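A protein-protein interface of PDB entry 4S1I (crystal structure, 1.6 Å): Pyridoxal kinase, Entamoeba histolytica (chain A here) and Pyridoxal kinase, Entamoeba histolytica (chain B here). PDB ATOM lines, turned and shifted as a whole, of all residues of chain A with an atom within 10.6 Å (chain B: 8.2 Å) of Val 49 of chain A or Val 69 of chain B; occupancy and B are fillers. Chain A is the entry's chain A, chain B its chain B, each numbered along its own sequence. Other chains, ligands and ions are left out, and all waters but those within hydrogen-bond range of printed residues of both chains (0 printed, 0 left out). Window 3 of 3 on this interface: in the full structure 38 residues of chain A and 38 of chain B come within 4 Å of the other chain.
The side-chain amide oxygen of Asn 43 of chain A sits at hydrogen-bond distance from the side-chain hydroxyl of Ser 66 of chain B (2.8 Å).
OG of Ser 66 of chain B lies within hydrogen-bond range of N of Gly 51 of chain A, 3.0 Å away.
O of Val 49 of chain A is in hydrogen-bond range of ND2 of Asn 70 of chain B (2.9 Å).
The side-chain amide oxygen of Asn 43 of chain A is in hydrogen-bond range of the side-chain amide nitrogen of Asn 70 of chain B (3.0 Å).
The side-chain hydroxyl of Ser 62 of chain B sits at hydrogen-bond distance from the backbone NH of Gly 52 of chain A (3.0 Å).
The side-chain hydroxyl (OG) of Ser 66 of chain B is in hydrogen-bond range of the backbone carbonyl oxygen (O) of Val 49 of chain A (3.3 Å).
The backbone carbonyl oxygen of Leu 67 of chain B is in hydrogen-bond range of the backbone NH of Leu 72 of chain B, 2.9 Å away.
N of His 40 of chain A sits at hydrogen-bond distance from O of Ser 53 of chain A (3.0 Å).
O of Gly 51 of chain A lies within hydrogen-bond range of N of Ala 42 of chain A (2.9 Å).
The backbone carbonyl oxygen (O) of Ser 66 of chain B is in hydrogen-bond range of the side-chain amide nitrogen (ND2) of Asn 70 of chain B, at 3.2 Å.
N of Ser 14 of chain A sits at hydrogen-bond distance from O of Ala 42 of chain A, 3.1 Å away.
ND2 of Asn 43 of chain A lies within hydrogen-bond range of O of Val 49 of chain A (3.1 Å).
Ile 63 of chain B touches Ala 42 of chain A (O to CB, 3.5 Å).
Ser 66 of chain B touches Ala 42 of chain A (CB to CB, 3.5 Å).
CD2 of Leu 67 of chain B touches O of Ala 42 of chain A (3.6 Å).
Asn 43 of chain A touches Leu 72 of chain B.
Tyr 47 of chain A touches Leu 72 of chain B.
OD1 of Asn 70 of chain B touches CD of Pro 48 of chain A (3.6 Å).
CA of Val 50 of chain A touches OG of Ser 66 of chain B, at 3.8 Å.
Ser 62 of chain B touches Gly 51 of chain A (OG to CA, 3.2 Å).
Gly 51 of chain A touches Ile 63 of chain B.
CG1 of Ile 63 of chain B touches CA of Gly 52 of chain A (3.7 Å).
Printed residues of chain B within 4 Å of His 40 of chain A: Ile 63.
Of the printed residues of chain B, Ala 42 of chain A touches Ile 63 (3.5 Å), Ser 66 (3.5 Å) and Leu 67 (3.6 Å).
Of the printed residues of chain B, Asn 43 of chain A touches Ser 66 (2.8 Å), Asn 70 (3.0 Å) and Leu 72 (3.6 Å).
Of the printed residues of chain B, Gly 51 of chain A touches Ser 62, Ile 63 and Ser 66.
Ser 53 of chain A touches none of the printed residues of chain B.
Ser 66 of chain B touches five residues of chain A.
Asn 70 of chain B touches just these residues of chain A: Asn 43 (3.0 Å), Tyr 47 (3.6 Å), Pro 48 (3.6 Å) and Val 49 (2.9 Å).
Arg 96 of chain B touches none of the printed residues of chain A.
The nearest printed residue of chain A that does not touch Val 69 of chain B is Pro 48 of chain A (6.6 Å).
The nearest printed residue of chain A that does not touch Leu 67 of chain B is Ser 14 of chain A (4.1 Å).
Of the 16 printed residues of chain A, 9 touch a printed residue of chain B.
Hydrophobic or aromatic side chains of chain A that line the printed part of chain B: His 40, Ala 42, Tyr 47, Pro 48 and Val 49.
Among the printed residues, 19 pairs touch across the chains.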
ATOM      1  N   VAL A  12       5.500 -15.899  19.549  1.00  0.00           N
ATOM      2  CA  VAL A  12       5.986 -16.168  20.917  1.00  0.00           C
ATOM      3  C   VAL A  12       5.406 -15.099  21.852  1.00  0.00           C
ATOM      4  O   VAL A  12       5.382 -13.883  21.501  1.00  0.00           O
ATOM      5  CB  VAL A  12       7.536 -16.187  21.003  1.00  0.00           C
ATOM      6  CG1 VAL A  12       8.093 -17.307  20.198  1.00  0.00           C
ATOM      7  CG2 VAL A  12       8.190 -14.891  20.512  1.00  0.00           C
ATOM      8  N   SER A  14       6.660 -14.029  24.730  1.00  0.00           N
ATOM      9  CA  SER A  14       7.809 -13.225  25.242  1.00  0.00           C
ATOM     10  C   SER A  14       8.852 -13.338  24.119  1.00  0.00           C
ATOM     11  O   SER A  14       9.101 -14.397  23.615  1.00  0.00           O
ATOM     12  CB  SER A  14       8.374 -13.810  26.543  1.00  0.00           C
ATOM     13  OG  SER A  14       9.443 -12.951  27.036  1.00  0.00           O
ATOM     14  N   HIS A  40       1.751 -20.859  18.943  1.00  0.00           N
ATOM     15  CA  HIS A  40       1.459 -20.018  20.113  1.00  0.00           C
ATOM     16  C   HIS A  40       2.343 -20.529  21.220  1.00  0.00           C
ATOM     17  O   HIS A  40       1.950 -21.429  21.992  1.00  0.00           O
ATOM     18  CB  HIS A  40       0.013 -19.973  20.485  1.00  0.00           C
ATOM     19  CG  HIS A  40      -0.371 -19.184  21.702  1.00  0.00           C
ATOM     20  ND1 HIS A  40      -1.428 -19.551  22.526  1.00  0.00           N
ATOM     21  CD2 HIS A  40       0.163 -18.085  22.263  1.00  0.00           C
ATOM     22  CE1 HIS A  40      -1.543 -18.657  23.508  1.00  0.00           C
ATOM     23  NE2 HIS A  40      -0.598 -17.740  23.348  1.00  0.00           N
ATOM     24  N   LEU A  41       3.567 -20.024  21.291  1.00  0.00           N
ATOM     25  CA  LEU A  41       4.546 -20.520  22.144  1.00  0.00           C
ATOM     26  C   LEU A  41       4.846 -19.469  23.258  1.00  0.00           C
ATOM     27  O   LEU A  41       4.704 -18.319  23.015  1.00  0.00           O
ATOM     28  CB  LEU A  41       5.858 -20.863  21.428  1.00  0.00           C
ATOM     29  CG  LEU A  41       5.766 -21.756  20.218  1.00  0.00           C
ATOM     30  CD1 LEU A  41       7.104 -21.912  19.567  1.00  0.00           C
ATOM     31  CD2 LEU A  41       5.204 -23.094  20.625  1.00  0.00           C
ATOM     32  N   ALA A  42       5.296 -19.904  24.411  1.00  0.00           N
ATOM     33  CA  ALA A  42       5.671 -19.003  25.493  1.00  0.00           C
ATOM     34  C   ALA A  42       6.846 -18.184  25.099  1.00  0.00           C
ATOM     35  O   ALA A  42       6.949 -16.993  25.443  1.00  0.00           O
ATOM     36  CB  ALA A  42       5.997 -19.781  26.746  1.00  0.00           C
ATOM     37  N   ASN A  43       7.761 -18.814  24.386  1.00  0.00           N
ATOM     38  CA  ASN A  43       9.079 -18.226  24.175  1.00  0.00           C
ATOM     39  C   ASN A  43       9.686 -18.951  22.953  1.00  0.00           C
ATOM     40  O   ASN A  43       9.144 -20.009  22.517  1.00  0.00           O
ATOM     41  CB  ASN A  43       9.939 -18.315  25.403  1.00  0.00           C
ATOM     42  CG  ASN A  43       9.900 -19.679  26.092  1.00  0.00           C
ATOM     43  OD1 ASN A  43       9.411 -19.795  27.172  1.00  0.00           O
ATOM     44  ND2 ASN A  43      10.500 -20.662  25.437  1.00  0.00           N
ATOM     45  N   HIS A  44      10.788 -18.461  22.397  1.00  0.00           N
ATOM     46  CA  HIS A  44      11.396 -19.122  21.251  1.00  0.00           C
ATOM     47  C   HIS A  44      12.004 -20.500  21.639  1.00  0.00           C
ATOM     48  O   HIS A  44      12.137 -20.875  22.788  1.00  0.00           O
ATOM     49  CB  HIS A  44      12.373 -18.229  20.477  1.00  0.00           C
ATOM     50  CG  HIS A  44      13.574 -17.832  21.223  1.00  0.00           C
ATOM     51  ND1 HIS A  44      14.546 -18.747  21.562  1.00  0.00           N
ATOM     52  CD2 HIS A  44      14.030 -16.630  21.640  1.00  0.00           C
ATOM     53  CE1 HIS A  44      15.535 -18.127  22.171  1.00  0.00           C
ATOM     54  NE2 HIS A  44      15.252 -16.829  22.192  1.00  0.00           N
ATOM     55  N   THR A  45      12.403 -21.214  20.581  1.00  0.00           N
ATOM     56  CA  THR A  45      12.860 -22.594  20.718  1.00  0.00           C
ATOM     57  C   THR A  45      14.271 -22.814  21.212  1.00  0.00           C
ATOM     58  O   THR A  45      14.673 -23.900  21.453  1.00  0.00           O
ATOM     59  CB  THR A  45      12.662 -23.411  19.399  1.00  0.00           C
ATOM     60  OG1 THR A  45      13.372 -22.784  18.333  1.00  0.00           O
ATOM     61  CG2 THR A  45      11.245 -23.486  19.068  1.00  0.00           C
ATOM     62  N   GLY A  46      15.016 -21.760  21.388  1.00  0.00           N
ATOM     63  CA  GLY A  46      16.275 -21.755  22.019  1.00  0.00           C
ATOM     64  C   GLY A  46      16.315 -21.964  23.513  1.00  0.00           C
ATOM     65  O   GLY A  46      17.392 -22.241  24.044  1.00  0.00           O
ATOM     66  N   TYR A  47      15.187 -21.927  24.220  1.00  0.00           N
ATOM     67  CA  TYR A  47      15.141 -22.150  25.622  1.00  0.00           C
ATOM     68  C   TYR A  47      14.998 -23.656  25.931  1.00  0.00           C
ATOM     69  O   TYR A  47      14.566 -24.394  25.088  1.00  0.00           O
ATOM     70  CB  TYR A  47      13.969 -21.422  26.325  1.00  0.00           C
ATOM     71  CG  TYR A  47      14.148 -19.951  26.357  1.00  0.00           C
ATOM     72  CD1 TYR A  47      13.766 -19.158  25.310  1.00  0.00           C
ATOM     73  CD2 TYR A  47      14.694 -19.341  27.484  1.00  0.00           C
ATOM     74  CE1 TYR A  47      13.932 -17.786  25.375  1.00  0.00           C
ATOM     75  CE2 TYR A  47      14.898 -17.988  27.508  1.00  0.00           C
ATOM     76  CZ  TYR A  47      14.491 -17.226  26.446  1.00  0.00           C
ATOM     77  OH  TYR A  47      14.695 -15.864  26.496  1.00  0.00           O
ATOM     78  N   PRO A  48      15.358 -24.066  27.149  1.00  0.00           N
ATOM     79  CA  PRO A  48      15.247 -25.509  27.417  1.00  0.00           C
ATOM     80  C   PRO A  48      13.819 -26.042  27.488  1.00  0.00           C
ATOM     81  O   PRO A  48      13.617 -27.225  27.321  1.00  0.00           O
ATOM     82  CB  PRO A  48      15.925 -25.693  28.771  1.00  0.00           C
ATOM     83  CG  PRO A  48      16.467 -24.358  29.161  1.00  0.00           C
ATOM     84  CD  PRO A  48      16.061 -23.318  28.218  1.00  0.00           C
ATOM     85  N   VAL A  49      12.864 -25.176  27.812  1.00  0.00           N
ATOM     86  CA  VAL A  49      11.443 -25.520  27.896  1.00  0.00           C
ATOM     87  C   VAL A  49      10.749 -24.591  26.929  1.00  0.00           C
ATOM     88  O   VAL A  49      11.097 -23.383  26.878  1.00  0.00           O
ATOM     89  CB  VAL A  49      10.974 -25.277  29.317  1.00  0.00           C
ATOM     90  CG1 VAL A  49       9.493 -25.536  29.472  1.00  0.00           C
ATOM     91  CG2 VAL A  49      11.713 -26.216  30.272  1.00  0.00           C
ATOM     92  N   VAL A  50       9.831 -25.141  26.110  1.00  0.00           N
ATOM     93  CA  VAL A  50       9.141 -24.343  25.135  1.00  0.00           C
ATOM     94  C   VAL A  50       7.674 -24.677  25.242  1.00  0.00           C
ATOM     95  O   VAL A  50       7.124 -25.478  24.472  1.00  0.00           O
ATOM     96  CB  VAL A  50       9.671 -24.541  23.675  1.00  0.00           C
ATOM     97  CG1 VAL A  50       8.977 -23.658  22.657  1.00  0.00           C
ATOM     98  CG2 VAL A  50      11.196 -24.524  23.610  1.00  0.00           C
ATOM     99  N   GLY A  51       6.991 -23.976  26.108  1.00  0.00           N
ATOM    100  CA  GLY A  51       5.565 -24.230  26.324  1.00  0.00           C
ATOM    101  C   GLY A  51       4.716 -23.761  25.183  1.00  0.00           C
ATOM    102  O   GLY A  51       5.033 -22.794  24.473  1.00  0.00           O
ATOM    103  N   GLY A  52       3.564 -24.400  25.035  1.00  0.00           N
ATOM    104  CA  GLY A  52       2.603 -24.067  23.976  1.00  0.00           C
ATOM    105  C   GLY A  52       2.717 -25.017  22.795  1.00  0.00           C
ATOM    106  O   GLY A  52       3.581 -25.862  22.766  1.00  0.00           O
ATOM    107  N   SER A  53       1.871 -24.784  21.806  1.00  0.00           N
ATOM    108  CA  SER A  53       1.707 -25.660  20.679  1.00  0.00           C
ATOM    109  C   SER A  53       1.838 -24.972  19.301  1.00  0.00           C
ATOM    110  O   SER A  53       1.585 -23.802  19.193  1.00  0.00           O
ATOM    111  CB  SER A  53       0.319 -26.302  20.722  1.00  0.00           C
ATOM    112  OG  SER A  53       0.301 -27.387  21.648  1.00  0.00           O
ATOM    113  N   SER B  62       0.799 -24.881  29.905  1.00  0.00           N
ATOM    114  CA  SER B  62       2.119 -25.098  29.337  1.00  0.00           C
ATOM    115  C   SER B  62       2.873 -23.779  29.097  1.00  0.00           C
ATOM    116  O   SER B  62       4.067 -23.662  29.426  1.00  0.00           O
ATOM    117  CB  SER B  62       2.001 -25.826  28.000  1.00  0.00           C
ATOM    118  OG  SER B  62       3.223 -26.122  27.446  1.00  0.00           O
ATOM    119  N   ILE B  63       2.180 -22.798  28.525  1.00  0.00           N
ATOM    120  CA  ILE B  63       2.795 -21.487  28.288  1.00  0.00           C
ATOM    121  C   ILE B  63       3.149 -20.862  29.633  1.00  0.00           C
ATOM    122  O   ILE B  63       4.275 -20.361  29.787  1.00  0.00           O
ATOM    123  CB  ILE B  63       1.795 -20.590  27.482  1.00  0.00           C
ATOM    124  CG1 ILE B  63       1.789 -21.165  26.090  1.00  0.00           C
ATOM    125  CG2 ILE B  63       2.153 -19.142  27.597  1.00  0.00           C
ATOM    126  CD1 ILE B  63       0.664 -20.629  25.262  1.00  0.00           C
ATOM    127  N   MET B  64       2.179 -20.800  30.558  1.00  0.00           N
ATOM    128  CA  MET B  64       2.484 -20.121  31.829  1.00  0.00           C
ATOM    129  C   MET B  64       3.680 -20.776  32.541  1.00  0.00           C
ATOM    130  O   MET B  64       4.559 -20.132  33.146  1.00  0.00           O
ATOM    131  CB  MET B  64       1.252 -20.002  32.708  1.00  0.00           C
ATOM    132  CG  MET B  64       0.113 -19.221  32.136  1.00  0.00           C
ATOM    133  SD  MET B  64       0.539 -17.473  31.751  1.00  0.00           S
ATOM    134  CE  MET B  64       0.681 -16.822  33.334  1.00  0.00           C
ATOM    135  N   ASP B  65       3.680 -22.109  32.531  1.00  0.00           N
ATOM    136  CA  ASP B  65       4.742 -22.864  33.137  1.00  0.00           C
ATOM    137  C   ASP B  65       6.096 -22.539  32.497  1.00  0.00           C
ATOM    138  O   ASP B  65       7.103 -22.426  33.196  1.00  0.00           O
ATOM    139  CB  ASP B  65       4.524 -24.364  33.090  1.00  0.00           C
ATOM    140  CG  ASP B  65       3.465 -24.859  34.068  1.00  0.00           C
ATOM    141  OD1 ASP B  65       2.919 -24.115  34.906  1.00  0.00           O
ATOM    142  OD2 ASP B  65       3.130 -26.052  33.924  1.00  0.00           O
ATOM    143  N   SER B  66       6.132 -22.456  31.185  1.00  0.00           N
ATOM    144  CA  SER B  66       7.343 -22.194  30.442  1.00  0.00           C
ATOM    145  C   SER B  66       7.857 -20.760  30.751  1.00  0.00           C
ATOM    146  O   SER B  66       9.087 -20.564  30.947  1.00  0.00           O
ATOM    147  CB  SER B  66       7.067 -22.246  28.915  1.00  0.00           C
ATOM    148  OG  SER B  66       8.269 -22.216  28.134  1.00  0.00           O
ATOM    149  N   LEU B  67       6.966 -19.796  30.864  1.00  0.00           N
ATOM    150  CA  LEU B  67       7.352 -18.397  31.219  1.00  0.00           C
ATOM    151  C   LEU B  67       8.076 -18.430  32.595  1.00  0.00           C
ATOM    152  O   LEU B  67       9.106 -17.779  32.789  1.00  0.00           O
ATOM    153  CB  LEU B  67       6.172 -17.468  31.280  1.00  0.00           C
ATOM    154  CG  LEU B  67       5.528 -17.203  29.898  1.00  0.00           C
ATOM    155  CD1 LEU B  67       4.285 -16.398  30.111  1.00  0.00           C
ATOM    156  CD2 LEU B  67       6.551 -16.473  29.023  1.00  0.00           C
ATOM    157  N   GLU B  68       7.486 -19.124  33.531  1.00  0.00           N
ATOM    158  CA  GLU B  68       8.043 -19.251  34.874  1.00  0.00           C
ATOM    159  C   GLU B  68       9.373 -19.934  34.934  1.00  0.00           C
ATOM    160  O   GLU B  68      10.324 -19.448  35.557  1.00  0.00           O
ATOM    161  CB  GLU B  68       7.032 -20.005  35.735  1.00  0.00           C
ATOM    162  CG  GLU B  68       7.384 -19.978  37.207  1.00  0.00           C
ATOM    163  CD  GLU B  68       6.264 -20.659  38.021  1.00  0.00           C
ATOM    164  OE1 GLU B  68       5.152 -20.995  37.424  1.00  0.00           O
ATOM    165  OE2 GLU B  68       6.531 -20.904  39.240  1.00  0.00           O
ATOM    166  N   VAL B  69       9.494 -21.098  34.309  1.00  0.00           N
ATOM    167  CA  VAL B  69      10.727 -21.937  34.359  1.00  0.00           C
ATOM    168  C   VAL B  69      11.930 -21.312  33.668  1.00  0.00           C
ATOM    169  O   VAL B  69      13.071 -21.469  34.078  1.00  0.00           O
ATOM    170  CB  VAL B  69      10.419 -23.314  33.753  1.00  0.00           C
ATOM    171  CG1 VAL B  69      11.641 -24.206  33.713  1.00  0.00           C
ATOM    172  CG2 VAL B  69       9.367 -23.999  34.610  1.00  0.00           C
ATOM    173  N   ASN B  70      11.642 -20.537  32.597  1.00  0.00           N
ATOM    174  CA  ASN B  70      12.685 -19.774  31.952  1.00  0.00           C
ATOM    175  C   ASN B  70      12.917 -18.385  32.529  1.00  0.00           C
ATOM    176  O   ASN B  70      13.711 -17.595  31.972  1.00  0.00           O
ATOM    177  CB  ASN B  70      12.305 -19.628  30.445  1.00  0.00           C
ATOM    178  CG  ASN B  70      12.356 -20.978  29.727  1.00  0.00           C
ATOM    179  OD1 ASN B  70      13.267 -21.763  29.934  1.00  0.00           O
ATOM    180  ND2 ASN B  70      11.403 -21.216  28.844  1.00  0.00           N
ATOM    181  N   HIS B  71      12.247 -18.032  33.602  1.00  0.00           N
ATOM    182  CA  HIS B  71      12.438 -16.776  34.329  1.00  0.00           C
ATOM    183  C   HIS B  71      12.010 -15.521  33.610  1.00  0.00           C
ATOM    184  O   HIS B  71      12.454 -14.412  33.951  1.00  0.00           O
ATOM    185  CB  HIS B  71      13.906 -16.720  34.831  1.00  0.00           C
ATOM    186  CG  HIS B  71      14.354 -17.963  35.447  1.00  0.00           C
ATOM    187  ND1 HIS B  71      13.945 -18.352  36.686  1.00  0.00           N
ATOM    188  CD2 HIS B  71      15.204 -18.918  35.015  1.00  0.00           C
ATOM    189  CE1 HIS B  71      14.543 -19.477  37.019  1.00  0.00           C
ATOM    190  NE2 HIS B  71      15.342 -19.820  36.026  1.00  0.00           N
ATOM    191  N   LEU B  72      11.135 -15.678  32.640  1.00  0.00           N
ATOM    192  CA  LEU B  72      10.764 -14.558  31.764  1.00  0.00           C
ATOM    193  C   LEU B  72       9.725 -13.669  32.428  1.00  0.00           C
ATOM    194  O   LEU B  72       9.520 -12.566  31.927  1.00  0.00           O
ATOM    195  CB  LEU B  72      10.235 -15.151  30.475  1.00  0.00           C
ATOM    196  CG  LEU B  72      11.276 -15.907  29.681  1.00  0.00           C
ATOM    197  CD1 LEU B  72      10.622 -16.525  28.447  1.00  0.00           C
ATOM    198  CD2 LEU B  72      12.408 -14.991  29.260  1.00  0.00           C
ATOM    199  N   ASP B  73       9.054 -14.124  33.487  1.00  0.00           N
ATOM    200  CA  ASP B  73       8.154 -13.334  34.266  1.00  0.00           C
ATOM    201  C   ASP B  73       8.644 -12.875  35.624  1.00  0.00           C
ATOM    202  O   ASP B  73       7.878 -12.306  36.423  1.00  0.00           O
ATOM    203  CB  ASP B  73       6.856 -14.096  34.449  1.00  0.00           C
ATOM    204  CG  ASP B  73       7.041 -15.353  35.279  1.00  0.00           C
ATOM    205  OD1 ASP B  73       8.201 -15.688  35.703  1.00  0.00           O
ATOM    206  OD2 ASP B  73       6.014 -16.024  35.479  1.00  0.00           O
ATOM    207  N   ARG B  96      -2.796 -18.474  38.810  1.00  0.00           N
ATOM    208  CA  ARG B  96      -1.557 -17.726  38.466  1.00  0.00           C
ATOM    209  C   ARG B  96      -1.468 -16.337  39.143  1.00  0.00           C
ATOM    210  O   ARG B  96      -0.436 -16.039  39.727  1.00  0.00           O
ATOM    211  CB  ARG B  96      -1.508 -17.533  36.986  1.00  0.00           C
ATOM    212  CG  ARG B  96      -1.396 -18.798  36.190  1.00  0.00           C
ATOM    213  CD  ARG B  96      -0.199 -19.684  36.486  1.00  0.00           C
ATOM    214  NE  ARG B  96      -0.342 -21.020  35.870  1.00  0.00           N
ATOM    215  CZ  ARG B  96       0.640 -21.905  35.609  1.00  0.00           C
ATOM    216  NH1 ARG B  96       1.906 -21.583  35.752  1.00  0.00           N
ATOM    217  NH2 ARG B  96       0.349 -23.103  35.121  1.00  0.00           N
